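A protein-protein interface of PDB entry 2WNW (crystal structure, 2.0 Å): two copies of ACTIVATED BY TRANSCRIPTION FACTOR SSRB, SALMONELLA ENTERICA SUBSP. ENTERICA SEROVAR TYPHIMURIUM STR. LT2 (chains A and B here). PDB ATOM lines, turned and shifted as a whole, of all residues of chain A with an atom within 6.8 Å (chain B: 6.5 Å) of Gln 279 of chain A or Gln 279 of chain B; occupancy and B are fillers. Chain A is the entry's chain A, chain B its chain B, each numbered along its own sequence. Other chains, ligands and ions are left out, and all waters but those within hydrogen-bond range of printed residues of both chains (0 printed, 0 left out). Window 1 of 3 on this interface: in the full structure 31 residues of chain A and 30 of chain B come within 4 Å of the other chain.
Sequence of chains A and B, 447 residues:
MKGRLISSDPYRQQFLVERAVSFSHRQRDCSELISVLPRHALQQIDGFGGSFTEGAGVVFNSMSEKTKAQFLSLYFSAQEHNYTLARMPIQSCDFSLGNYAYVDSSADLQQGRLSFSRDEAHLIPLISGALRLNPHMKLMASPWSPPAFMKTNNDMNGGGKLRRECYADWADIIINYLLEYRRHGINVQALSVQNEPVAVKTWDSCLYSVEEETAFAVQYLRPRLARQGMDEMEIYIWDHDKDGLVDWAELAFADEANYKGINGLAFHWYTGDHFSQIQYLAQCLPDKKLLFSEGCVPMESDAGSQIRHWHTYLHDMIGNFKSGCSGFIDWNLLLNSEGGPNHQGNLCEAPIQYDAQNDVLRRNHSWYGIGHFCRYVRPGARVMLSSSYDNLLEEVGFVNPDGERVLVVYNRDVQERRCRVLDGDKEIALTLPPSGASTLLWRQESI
The side-chain hydroxyl (OG) of Ser 276 of chain A lies within hydrogen-bond range of the side-chain amino group (NZ) of Lys 322 of chain B, 2.9 Å away.
The side-chain amide nitrogen (NE2) of Gln 283 of chain A lies close to the side-chain amide nitrogen (NE2) of Gln 279 of chain B, at 3.3 Å.
The side-chain amide nitrogen of Gln 283 of chain B sits close to the side-chain amide nitrogen of Gln 283 of chain A, at 2.8 Å.
The side-chain amino group (NZ) of Lys 322 of chain A is in hydrogen-bond range of the side-chain hydroxyl (OG) of Ser 276 of chain B (3.0 Å).
The backbone NH (N) of Gln 279 of chain A sits close to the backbone carbonyl oxygen (O) of Ser 323 of chain A (3.2 Å).
The backbone carbonyl oxygen of Ser 323 of chain B sits close to the backbone NH of Gln 279 of chain B (3.3 Å).
The backbone carbonyl oxygen (O) of Tyr 280 of chain B is in hydrogen-bond range of the side-chain sulfur (SG) of Cys 284 of chain B (3.3 Å).
Among the printed residues, pairs that only touch across the chains: Leu 385 of chain A with Tyr 280 of chain B (3.6 Å) and Gln 279 of chain A with Gln 279 of chain B (3.8 Å).
Of chain B, only Gln 279 comes within 4 Å of Gln 279 of chain A.
Ser 323 of chain A touches none of the printed residues of chain B.
Of the printed residues of chain A, Ser 276 of chain B touches Lys 322 (3.0 Å).
Gln 279 of chain B touches just these residues of chain A: Gln 279 (3.8 Å) and Gln 283 (3.3 Å).
Printed residues of chain A within 4 Å of Lys 322 of chain B: Ser 276 (2.9 Å).
The nearest residue of chain A that does not touch Gln 279 of chain B is Leu 385 of chain A (6.6 Å).
Printed residues of chain A that touch a printed residue of chain B: Ser 276, Gln 279, Gln 283, Lys 322 and Leu 385.
Hydrophobic or aromatic side chains of chain A that line the printed part of chain B: Leu 385.
Of the 15 printed residues of chain B, 5 touch a printed residue of chain A.
Along chain B the printed residues that touch a printed residue of chain A span positions 276 to 322.
Among the printed residues, no Asp or Glu carboxylate lies within 4 Å of a Lys or Arg side-chain nitrogen of the other chain.
Ser 276 of chain A touches Lys 322 of chain B, and with the chains exchanged Lys 322 of chain A touches Ser 276 of chain B.
Gln 279 of chain B touches its own counterpart, Gln 279 of chain A.
Gln 283 of chain A touches Gln 279 of chain B, but with the chains exchanged Gln 279 of chain A does not touch Gln 283 of chain B (6.6 Å).
Gln 283 of chain A touches its own counterpart, Gln 283 of chain B.
Positions printed for both chains: 274, 275, 276, 277, 278, 279, 280, 281, 282, 283, 284, 290, 322, 323 and 324.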
ATOM      1  N   LEU A 245      -5.454 -13.236  21.684  1.00  0.00           N
ATOM      2  CA  LEU A 245      -6.539 -12.436  22.242  1.00  0.00           C
ATOM      3  C   LEU A 245      -6.586 -12.322  23.773  1.00  0.00           C
ATOM      4  O   LEU A 245      -6.574 -11.216  24.325  1.00  0.00           O
ATOM      5  CB  LEU A 245      -7.865 -12.993  21.721  1.00  0.00           C
ATOM      6  CG  LEU A 245      -9.090 -12.092  21.605  1.00  0.00           C
ATOM      7  CD1 LEU A 245      -8.733 -10.799  20.893  1.00  0.00           C
ATOM      8  CD2 LEU A 245     -10.175 -12.849  20.838  1.00  0.00           C
ATOM      9  N   HIS A 274      -9.715 -20.562  17.027  1.00  0.00           N
ATOM     10  CA  HIS A 274      -9.495 -20.062  18.384  1.00  0.00           C
ATOM     11  C   HIS A 274     -10.746 -19.407  18.966  1.00  0.00           C
ATOM     12  O   HIS A 274     -10.661 -18.413  19.685  1.00  0.00           O
ATOM     13  CB  HIS A 274      -8.329 -19.068  18.388  1.00  0.00           C
ATOM     14  CG  HIS A 274      -7.006 -19.701  18.088  1.00  0.00           C
ATOM     15  ND1 HIS A 274      -6.421 -20.628  18.924  1.00  0.00           N
ATOM     16  CD2 HIS A 274      -6.172 -19.573  17.028  1.00  0.00           C
ATOM     17  CE1 HIS A 274      -5.287 -21.045  18.392  1.00  0.00           C
ATOM     18  NE2 HIS A 274      -5.112 -20.421  17.240  1.00  0.00           N
ATOM     19  N   PHE A 275     -11.908 -19.982  18.672  1.00  0.00           N
ATOM     20  CA  PHE A 275     -13.171 -19.425  19.149  1.00  0.00           C
ATOM     21  C   PHE A 275     -13.262 -19.324  20.672  1.00  0.00           C
ATOM     22  O   PHE A 275     -13.884 -18.404  21.200  1.00  0.00           O
ATOM     23  CB  PHE A 275     -14.355 -20.252  18.620  1.00  0.00           C
ATOM     24  CG  PHE A 275     -14.408 -20.357  17.111  1.00  0.00           C
ATOM     25  CD1 PHE A 275     -14.350 -19.215  16.313  1.00  0.00           C
ATOM     26  CD2 PHE A 275     -14.527 -21.599  16.494  1.00  0.00           C
ATOM     27  CE1 PHE A 275     -14.409 -19.311  14.915  1.00  0.00           C
ATOM     28  CE2 PHE A 275     -14.586 -21.712  15.098  1.00  0.00           C
ATOM     29  CZ  PHE A 275     -14.526 -20.563  14.307  1.00  0.00           C
ATOM     30  N   SER A 276     -12.645 -20.269  21.375  1.00  0.00           N
ATOM     31  CA  SER A 276     -12.683 -20.274  22.835  1.00  0.00           C
ATOM     32  C   SER A 276     -12.148 -18.996  23.478  1.00  0.00           C
ATOM     33  O   SER A 276     -12.597 -18.614  24.562  1.00  0.00           O
ATOM     34  CB  SER A 276     -11.913 -21.480  23.384  1.00  0.00           C
ATOM     35  OG  SER A 276     -12.616 -22.685  23.143  1.00  0.00           O
ATOM     36  N   GLN A 277     -11.196 -18.333  22.825  1.00  0.00           N
ATOM     37  CA  GLN A 277     -10.645 -17.106  23.392  1.00  0.00           C
ATOM     38  C   GLN A 277     -11.640 -15.957  23.300  1.00  0.00           C
ATOM     39  O   GLN A 277     -11.657 -15.074  24.157  1.00  0.00           O
ATOM     40  CB  GLN A 277      -9.315 -16.748  22.718  1.00  0.00           C
ATOM     41  CG  GLN A 277      -8.205 -17.726  23.103  1.00  0.00           C
ATOM     42  CD  GLN A 277      -6.818 -17.208  22.802  1.00  0.00           C
ATOM     43  OE1 GLN A 277      -6.506 -16.046  23.066  1.00  0.00           O
ATOM     44  NE2 GLN A 277      -5.966 -18.078  22.263  1.00  0.00           N
ATOM     45  N   ILE A 278     -12.476 -15.972  22.268  1.00  0.00           N
ATOM     46  CA  ILE A 278     -13.497 -14.938  22.128  1.00  0.00           C
ATOM     47  C   ILE A 278     -14.510 -15.158  23.250  1.00  0.00           C
ATOM     48  O   ILE A 278     -14.879 -14.226  23.964  1.00  0.00           O
ATOM     49  CB  ILE A 278     -14.254 -15.047  20.792  1.00  0.00           C
ATOM     50  CG1 ILE A 278     -13.287 -14.917  19.616  1.00  0.00           C
ATOM     51  CG2 ILE A 278     -15.312 -13.945  20.710  1.00  0.00           C
ATOM     52  CD1 ILE A 278     -13.960 -15.127  18.279  1.00  0.00           C
ATOM     53  N   GLN A 279     -14.942 -16.408  23.405  1.00  0.00           N
ATOM     54  CA  GLN A 279     -15.922 -16.761  24.429  1.00  0.00           C
ATOM     55  C   GLN A 279     -15.467 -16.441  25.851  1.00  0.00           C
ATOM     56  O   GLN A 279     -16.253 -15.938  26.657  1.00  0.00           O
ATOM     57  CB  GLN A 279     -16.282 -18.243  24.326  1.00  0.00           C
ATOM     58  CG  GLN A 279     -17.404 -18.648  25.262  1.00  0.00           C
ATOM     59  CD  GLN A 279     -18.183 -19.830  24.742  1.00  0.00           C
ATOM     60  OE1 GLN A 279     -17.662 -20.944  24.658  1.00  0.00           O
ATOM     61  NE2 GLN A 279     -19.439 -19.594  24.374  1.00  0.00           N
ATOM     62  N   TYR A 280     -14.206 -16.726  26.158  1.00  0.00           N
ATOM     63  CA  TYR A 280     -13.678 -16.445  27.491  1.00  0.00           C
ATOM     64  C   TYR A 280     -13.752 -14.943  27.776  1.00  0.00           C
ATOM     65  O   TYR A 280     -14.174 -14.528  28.854  1.00  0.00           O
ATOM     66  CB  TYR A 280     -12.222 -16.910  27.607  1.00  0.00           C
ATOM     67  CG  TYR A 280     -11.652 -16.793  29.010  1.00  0.00           C
ATOM     68  CD1 TYR A 280     -12.085 -17.636  30.035  1.00  0.00           C
ATOM     69  CD2 TYR A 280     -10.682 -15.838  29.312  1.00  0.00           C
ATOM     70  CE1 TYR A 280     -11.566 -17.532  31.325  1.00  0.00           C
ATOM     71  CE2 TYR A 280     -10.156 -15.725  30.599  1.00  0.00           C
ATOM     72  CZ  TYR A 280     -10.601 -16.574  31.599  1.00  0.00           C
ATOM     73  OH  TYR A 280     -10.082 -16.468  32.871  1.00  0.00           O
ATOM     74  N   LEU A 281     -13.333 -14.129  26.813  1.00  0.00           N
ATOM     75  CA  LEU A 281     -13.369 -12.682  27.001  1.00  0.00           C
ATOM     76  C   LEU A 281     -14.800 -12.160  27.048  1.00  0.00           C
ATOM     77  O   LEU A 281     -15.087 -11.164  27.716  1.00  0.00           O
ATOM     78  CB  LEU A 281     -12.595 -11.968  25.884  1.00  0.00           C
ATOM     79  CG  LEU A 281     -11.072 -12.152  25.858  1.00  0.00           C
ATOM     80  CD1 LEU A 281     -10.478 -11.164  24.857  1.00  0.00           C
ATOM     81  CD2 LEU A 281     -10.476 -11.908  27.241  1.00  0.00           C
ATOM     82  N   ALA A 282     -15.700 -12.830  26.334  1.00  0.00           N
ATOM     83  CA  ALA A 282     -17.097 -12.418  26.320  1.00  0.00           C
ATOM     84  C   ALA A 282     -17.690 -12.614  27.715  1.00  0.00           C
ATOM     85  O   ALA A 282     -18.573 -11.868  28.134  1.00  0.00           O
ATOM     86  CB  ALA A 282     -17.878 -13.236  25.298  1.00  0.00           C
ATOM     87  N   GLN A 283     -17.195 -13.615  28.431  1.00  0.00           N
ATOM     88  CA  GLN A 283     -17.688 -13.897  29.775  1.00  0.00           C
ATOM     89  C   GLN A 283     -16.981 -13.036  30.824  1.00  0.00           C
ATOM     90  O   GLN A 283     -17.594 -12.623  31.807  1.00  0.00           O
ATOM     91  CB  GLN A 283     -17.507 -15.387  30.089  1.00  0.00           C
ATOM     92  CG  GLN A 283     -18.168 -16.299  29.055  1.00  0.00           C
ATOM     93  CD  GLN A 283     -17.825 -17.769  29.239  1.00  0.00           C
ATOM     94  OE1 GLN A 283     -16.667 -18.129  29.465  1.00  0.00           O
ATOM     95  NE2 GLN A 283     -18.833 -18.631  29.121  1.00  0.00           N
ATOM     96  N   CYS A 284     -15.697 -12.756  30.603  1.00  0.00           N
ATOM     97  CA  CYS A 284     -14.908 -11.949  31.531  1.00  0.00           C
ATOM     98  C   CYS A 284     -15.082 -10.441  31.346  1.00  0.00           C
ATOM     99  O   CYS A 284     -14.996  -9.677  32.308  1.00  0.00           O
ATOM    100  CB  CYS A 284     -13.423 -12.305  31.404  1.00  0.00           C
ATOM    101  SG  CYS A 284     -13.015 -13.968  31.989  1.00  0.00           S
ATOM    102  N   LEU A 290     -16.054  -7.296  21.198  1.00  0.00           N
ATOM    103  CA  LEU A 290     -15.077  -8.175  20.564  1.00  0.00           C
ATOM    104  C   LEU A 290     -15.426  -8.186  19.081  1.00  0.00           C
ATOM    105  O   LEU A 290     -16.220  -8.998  18.614  1.00  0.00           O
ATOM    106  CB  LEU A 290     -15.172  -9.580  21.160  1.00  0.00           C
ATOM    107  CG  LEU A 290     -14.987  -9.618  22.683  1.00  0.00           C
ATOM    108  CD1 LEU A 290     -15.204 -11.038  23.194  1.00  0.00           C
ATOM    109  CD2 LEU A 290     -13.592  -9.123  23.052  1.00  0.00           C
ATOM    110  N   ASN A 320     -17.417 -17.151  15.358  1.00  0.00           N
ATOM    111  CA  ASN A 320     -17.210 -15.880  16.040  1.00  0.00           C
ATOM    112  C   ASN A 320     -18.478 -15.421  16.748  1.00  0.00           C
ATOM    113  O   ASN A 320     -18.459 -15.122  17.939  1.00  0.00           O
ATOM    114  CB  ASN A 320     -16.768 -14.798  15.043  1.00  0.00           C
ATOM    115  CG  ASN A 320     -15.333 -14.976  14.584  1.00  0.00           C
ATOM    116  OD1 ASN A 320     -14.866 -14.280  13.681  1.00  0.00           O
ATOM    117  ND2 ASN A 320     -14.627 -15.902  15.205  1.00  0.00           N
ATOM    118  N   LYS A 322     -21.170 -17.153  17.559  1.00  0.00           N
ATOM    119  CA  LYS A 322     -21.616 -18.077  18.597  1.00  0.00           C
ATOM    120  C   LYS A 322     -20.765 -17.868  19.846  1.00  0.00           C
ATOM    121  O   LYS A 322     -21.202 -18.147  20.961  1.00  0.00           O
ATOM    122  CB  LYS A 322     -21.470 -19.532  18.143  1.00  0.00           C
ATOM    123  CG  LYS A 322     -22.488 -19.969  17.113  1.00  0.00           C
ATOM    124  CD  LYS A 322     -23.294 -21.165  17.609  1.00  0.00           C
ATOM    125  CE  LYS A 322     -24.098 -20.834  18.849  1.00  0.00           C
ATOM    126  NZ  LYS A 322     -24.868 -22.015  19.360  1.00  0.00           N
ATOM    127  N   SER A 323     -19.550 -17.363  19.651  1.00  0.00           N
ATOM    128  CA  SER A 323     -18.621 -17.155  20.757  1.00  0.00           C
ATOM    129  C   SER A 323     -18.601 -15.775  21.417  1.00  0.00           C
ATOM    130  O   SER A 323     -17.830 -15.561  22.349  1.00  0.00           O
ATOM    131  CB  SER A 323     -17.209 -17.521  20.301  1.00  0.00           C
ATOM    132  OG  SER A 323     -17.196 -18.853  19.817  1.00  0.00           O
ATOM    133  N   GLY A 324     -19.418 -14.841  20.934  1.00  0.00           N
ATOM    134  CA  GLY A 324     -19.464 -13.525  21.557  1.00  0.00           C
ATOM    135  C   GLY A 324     -19.058 -12.319  20.723  1.00  0.00           C
ATOM    136  O   GLY A 324     -18.969 -11.210  21.254  1.00  0.00           O
ATOM    137  N   CYS A 325     -18.827 -12.529  19.428  1.00  0.00           N
ATOM    138  CA  CYS A 325     -18.412 -11.468  18.505  1.00  0.00           C
ATOM    139  C   CYS A 325     -19.452 -10.354  18.368  1.00  0.00           C
ATOM    140  O   CYS A 325     -20.648 -10.623  18.279  1.00  0.00           O
ATOM    141  CB  CYS A 325     -18.124 -12.075  17.126  1.00  0.00           C
ATOM    142  SG  CYS A 325     -17.563 -10.899  15.882  1.00  0.00           S
ATOM    143  N   LEU A 385     -29.632 -17.836  22.002  1.00  0.00           N
ATOM    144  CA  LEU A 385     -29.122 -19.135  22.404  1.00  0.00           C
ATOM    145  C   LEU A 385     -29.683 -20.181  21.447  1.00  0.00           C
ATOM    146  O   LEU A 385     -30.864 -20.147  21.100  1.00  0.00           O
ATOM    147  CB  LEU A 385     -29.571 -19.466  23.831  1.00  0.00           C
ATOM    148  CG  LEU A 385     -29.280 -20.890  24.311  1.00  0.00           C
ATOM    149  CD1 LEU A 385     -27.769 -21.080  24.444  1.00  0.00           C
ATOM    150  CD2 LEU A 385     -29.970 -21.141  25.650  1.00  0.00           C
ATOM    151  N   HIS B 274     -25.420 -30.742  21.150  1.00  0.00           N
ATOM    152  CA  HIS B 274     -26.102 -29.690  21.904  1.00  0.00           C
ATOM    153  C   HIS B 274     -25.207 -29.120  23.005  1.00  0.00           C
ATOM    154  O   HIS B 274     -25.677 -28.794  24.091  1.00  0.00           O
ATOM    155  CB  HIS B 274     -27.407 -30.238  22.509  1.00  0.00           C
ATOM    156  CG  HIS B 274     -28.452 -30.559  21.487  1.00  0.00           C
ATOM    157  ND1 HIS B 274     -29.069 -29.589  20.725  1.00  0.00           N
ATOM    158  CD2 HIS B 274     -28.953 -31.744  21.061  1.00  0.00           C
ATOM    159  CE1 HIS B 274     -29.900 -30.161  19.872  1.00  0.00           C
ATOM    160  NE2 HIS B 274     -29.849 -31.468  20.055  1.00  0.00           N
ATOM    161  N   PHE B 275     -23.915 -28.984  22.715  1.00  0.00           N
ATOM    162  CA  PHE B 275     -22.976 -28.478  23.712  1.00  0.00           C
ATOM    163  C   PHE B 275     -23.312 -27.081  24.232  1.00  0.00           C
ATOM    164  O   PHE B 275     -23.042 -26.769  25.392  1.00  0.00           O
ATOM    165  CB  PHE B 275     -21.545 -28.480  23.153  1.00  0.00           C
ATOM    166  CG  PHE B 275     -21.079 -29.827  22.678  1.00  0.00           C
ATOM    167  CD1 PHE B 275     -21.159 -30.945  23.508  1.00  0.00           C
ATOM    168  CD2 PHE B 275     -20.537 -29.978  21.406  1.00  0.00           C
ATOM    169  CE1 PHE B 275     -20.703 -32.195  23.077  1.00  0.00           C
ATOM    170  CE2 PHE B 275     -20.078 -31.223  20.966  1.00  0.00           C
ATOM    171  CZ  PHE B 275     -20.162 -32.331  21.804  1.00  0.00           C
ATOM    172  N   SER B 276     -23.901 -26.244  23.382  1.00  0.00           N
ATOM    173  CA  SER B 276     -24.247 -24.881  23.788  1.00  0.00           C
ATOM    174  C   SER B 276     -25.168 -24.816  25.001  1.00  0.00           C
ATOM    175  O   SER B 276     -25.073 -23.888  25.806  1.00  0.00           O
ATOM    176  CB  SER B 276     -24.895 -24.119  22.626  1.00  0.00           C
ATOM    177  OG  SER B 276     -23.960 -23.882  21.588  1.00  0.00           O
ATOM    178  N   GLN B 277     -26.067 -25.783  25.139  1.00  0.00           N
ATOM    179  CA  GLN B 277     -26.969 -25.753  26.280  1.00  0.00           C
ATOM    180  C   GLN B 277     -26.219 -25.990  27.585  1.00  0.00           C
ATOM    181  O   GLN B 277     -26.577 -25.428  28.621  1.00  0.00           O
ATOM    182  CB  GLN B 277     -28.113 -26.754  26.090  1.00  0.00           C
ATOM    183  CG  GLN B 277     -29.058 -26.319  24.967  1.00  0.00           C
ATOM    184  CD  GLN B 277     -30.406 -27.009  25.009  1.00  0.00           C
ATOM    185  OE1 GLN B 277     -31.009 -27.147  26.072  1.00  0.00           O
ATOM    186  NE2 GLN B 277     -30.894 -27.430  23.845  1.00  0.00           N
ATOM    187  N   ILE B 278     -25.169 -26.808  27.540  1.00  0.00           N
ATOM    188  CA  ILE B 278     -24.377 -27.048  28.744  1.00  0.00           C
ATOM    189  C   ILE B 278     -23.673 -25.738  29.091  1.00  0.00           C
ATOM    190  O   ILE B 278     -23.689 -25.285  30.240  1.00  0.00           O
ATOM    191  CB  ILE B 278     -23.282 -28.124  28.518  1.00  0.00           C
ATOM    192  CG1 ILE B 278     -23.915 -29.446  28.080  1.00  0.00           C
ATOM    193  CG2 ILE B 278     -22.479 -28.323  29.800  1.00  0.00           C
ATOM    194  CD1 ILE B 278     -22.893 -30.523  27.744  1.00  0.00           C
ATOM    195  N   GLN B 279     -23.055 -25.127  28.084  1.00  0.00           N
ATOM    196  CA  GLN B 279     -22.326 -23.881  28.286  1.00  0.00           C
ATOM    197  C   GLN B 279     -23.214 -22.770  28.840  1.00  0.00           C
ATOM    198  O   GLN B 279     -22.795 -22.012  29.718  1.00  0.00           O
ATOM    199  CB  GLN B 279     -21.681 -23.428  26.973  1.00  0.00           C
ATOM    200  CG  GLN B 279     -20.799 -22.184  27.111  1.00  0.00           C
ATOM    201  CD  GLN B 279     -19.597 -22.413  28.013  1.00  0.00           C
ATOM    202  OE1 GLN B 279     -18.657 -23.126  27.651  1.00  0.00           O
ATOM    203  NE2 GLN B 279     -19.624 -21.814  29.201  1.00  0.00           N
ATOM    204  N   TYR B 280     -24.440 -22.673  28.337  1.00  0.00           N
ATOM    205  CA  TYR B 280     -25.355 -21.640  28.807  1.00  0.00           C
ATOM    206  C   TYR B 280     -25.643 -21.825  30.297  1.00  0.00           C
ATOM    207  O   TYR B 280     -25.621 -20.862  31.064  1.00  0.00           O
ATOM    208  CB  TYR B 280     -26.665 -21.676  28.019  1.00  0.00           C
ATOM    209  CG  TYR B 280     -27.588 -20.519  28.335  1.00  0.00           C
ATOM    210  CD1 TYR B 280     -27.304 -19.233  27.879  1.00  0.00           C
ATOM    211  CD2 TYR B 280     -28.740 -20.710  29.098  1.00  0.00           C
ATOM    212  CE1 TYR B 280     -28.147 -18.161  28.171  1.00  0.00           C
ATOM    213  CE2 TYR B 280     -29.590 -19.645  29.398  1.00  0.00           C
ATOM    214  CZ  TYR B 280     -29.287 -18.376  28.931  1.00  0.00           C
ATOM    215  OH  TYR B 280     -30.124 -17.321  29.215  1.00  0.00           O
ATOM    216  N   LEU B 281     -25.903 -23.063  30.709  1.00  0.00           N
ATOM    217  CA  LEU B 281     -26.179 -23.336  32.116  1.00  0.00           C
ATOM    218  C   LEU B 281     -24.936 -23.158  32.984  1.00  0.00           C
ATOM    219  O   LEU B 281     -25.031 -22.719  34.135  1.00  0.00           O
ATOM    220  CB  LEU B 281     -26.743 -24.750  32.291  1.00  0.00           C
ATOM    221  CG  LEU B 281     -28.139 -24.963  31.693  1.00  0.00           C
ATOM    222  CD1 LEU B 281     -28.636 -26.360  32.038  1.00  0.00           C
ATOM    223  CD2 LEU B 281     -29.103 -23.912  32.235  1.00  0.00           C
ATOM    224  N   ALA B 282     -23.772 -23.493  32.438  1.00  0.00           N
ATOM    225  CA  ALA B 282     -22.527 -23.340  33.186  1.00  0.00           C
ATOM    226  C   ALA B 282     -22.347 -21.866  33.538  1.00  0.00           C
ATOM    227  O   ALA B 282     -21.794 -21.525  34.585  1.00  0.00           O
ATOM    228  CB  ALA B 282     -21.346 -23.833  32.356  1.00  0.00           C
ATOM    229  N   GLN B 283     -22.823 -20.991  32.658  1.00  0.00           N
ATOM    230  CA  GLN B 283     -22.728 -19.553  32.887  1.00  0.00           C
ATOM    231  C   GLN B 283     -23.812 -19.036  33.830  1.00  0.00           C
ATOM    232  O   GLN B 283     -23.535 -18.225  34.717  1.00  0.00           O
ATOM    233  CB  GLN B 283     -22.810 -18.801  31.558  1.00  0.00           C
ATOM    234  CG  GLN B 283     -21.497 -18.734  30.808  1.00  0.00           C
ATOM    235  CD  GLN B 283     -20.480 -17.847  31.508  1.00  0.00           C
ATOM    236  OE1 GLN B 283     -20.712 -16.651  31.706  1.00  0.00           O
ATOM    237  NE2 GLN B 283     -19.346 -18.429  31.884  1.00  0.00           N
ATOM    238  N   CYS B 284     -25.040 -19.510  33.636  1.00  0.00           N
ATOM    239  CA  CYS B 284     -26.179 -19.088  34.452  1.00  0.00           C
ATOM    240  C   CYS B 284     -26.262 -19.751  35.827  1.00  0.00           C
ATOM    241  O   CYS B 284     -26.807 -19.168  36.767  1.00  0.00           O
ATOM    242  CB  CYS B 284     -27.485 -19.344  33.694  1.00  0.00           C
ATOM    243  SG  CYS B 284     -27.619 -18.461  32.125  1.00  0.00           S
ATOM    244  N   LEU B 290     -23.157 -29.933  36.345  1.00  0.00           N
ATOM    245  CA  LEU B 290     -23.728 -30.424  35.096  1.00  0.00           C
ATOM    246  C   LEU B 290     -23.026 -31.744  34.803  1.00  0.00           C
ATOM    247  O   LEU B 290     -21.966 -31.785  34.178  1.00  0.00           O
ATOM    248  CB  LEU B 290     -23.480 -29.407  33.980  1.00  0.00           C
ATOM    249  CG  LEU B 290     -23.987 -28.009  34.344  1.00  0.00           C
ATOM    250  CD1 LEU B 290     -23.558 -26.995  33.292  1.00  0.00           C
ATOM    251  CD2 LEU B 290     -25.508 -28.046  34.479  1.00  0.00           C
ATOM    252  N   LYS B 322     -15.467 -29.164  27.654  1.00  0.00           N
ATOM    253  CA  LYS B 322     -15.116 -27.833  27.174  1.00  0.00           C
ATOM    254  C   LYS B 322     -16.272 -26.888  27.479  1.00  0.00           C
ATOM    255  O   LYS B 322     -16.083 -25.682  27.623  1.00  0.00           O
ATOM    256  CB  LYS B 322     -14.893 -27.843  25.657  1.00  0.00           C
ATOM    257  CG  LYS B 322     -13.512 -28.277  25.216  1.00  0.00           C
ATOM    258  CD  LYS B 322     -12.480 -27.173  25.423  1.00  0.00           C
ATOM    259  CE  LYS B 322     -12.690 -26.016  24.452  1.00  0.00           C
ATOM    260  NZ  LYS B 322     -11.584 -25.010  24.538  1.00  0.00           N
ATOM    261  N   SER B 323     -17.468 -27.457  27.592  1.00  0.00           N
ATOM    262  CA  SER B 323     -18.674 -26.672  27.815  1.00  0.00           C
ATOM    263  C   SER B 323     -19.169 -26.495  29.248  1.00  0.00           C
ATOM    264  O   SER B 323     -20.146 -25.780  29.464  1.00  0.00           O
ATOM    265  CB  SER B 323     -19.802 -27.249  26.957  1.00  0.00           C
ATOM    266  OG  SER B 323     -19.413 -27.280  25.594  1.00  0.00           O
ATOM    267  N   GLY B 324     -18.523 -27.135  30.220  1.00  0.00           N
ATOM    268  CA  GLY B 324     -18.947 -26.963  31.603  1.00  0.00           C
ATOM    269  C   GLY B 324     -19.281 -28.213  32.403  1.00  0.00           C
ATOM    270  O   GLY B 324     -19.610 -28.120  33.584  1.00  0.00           O
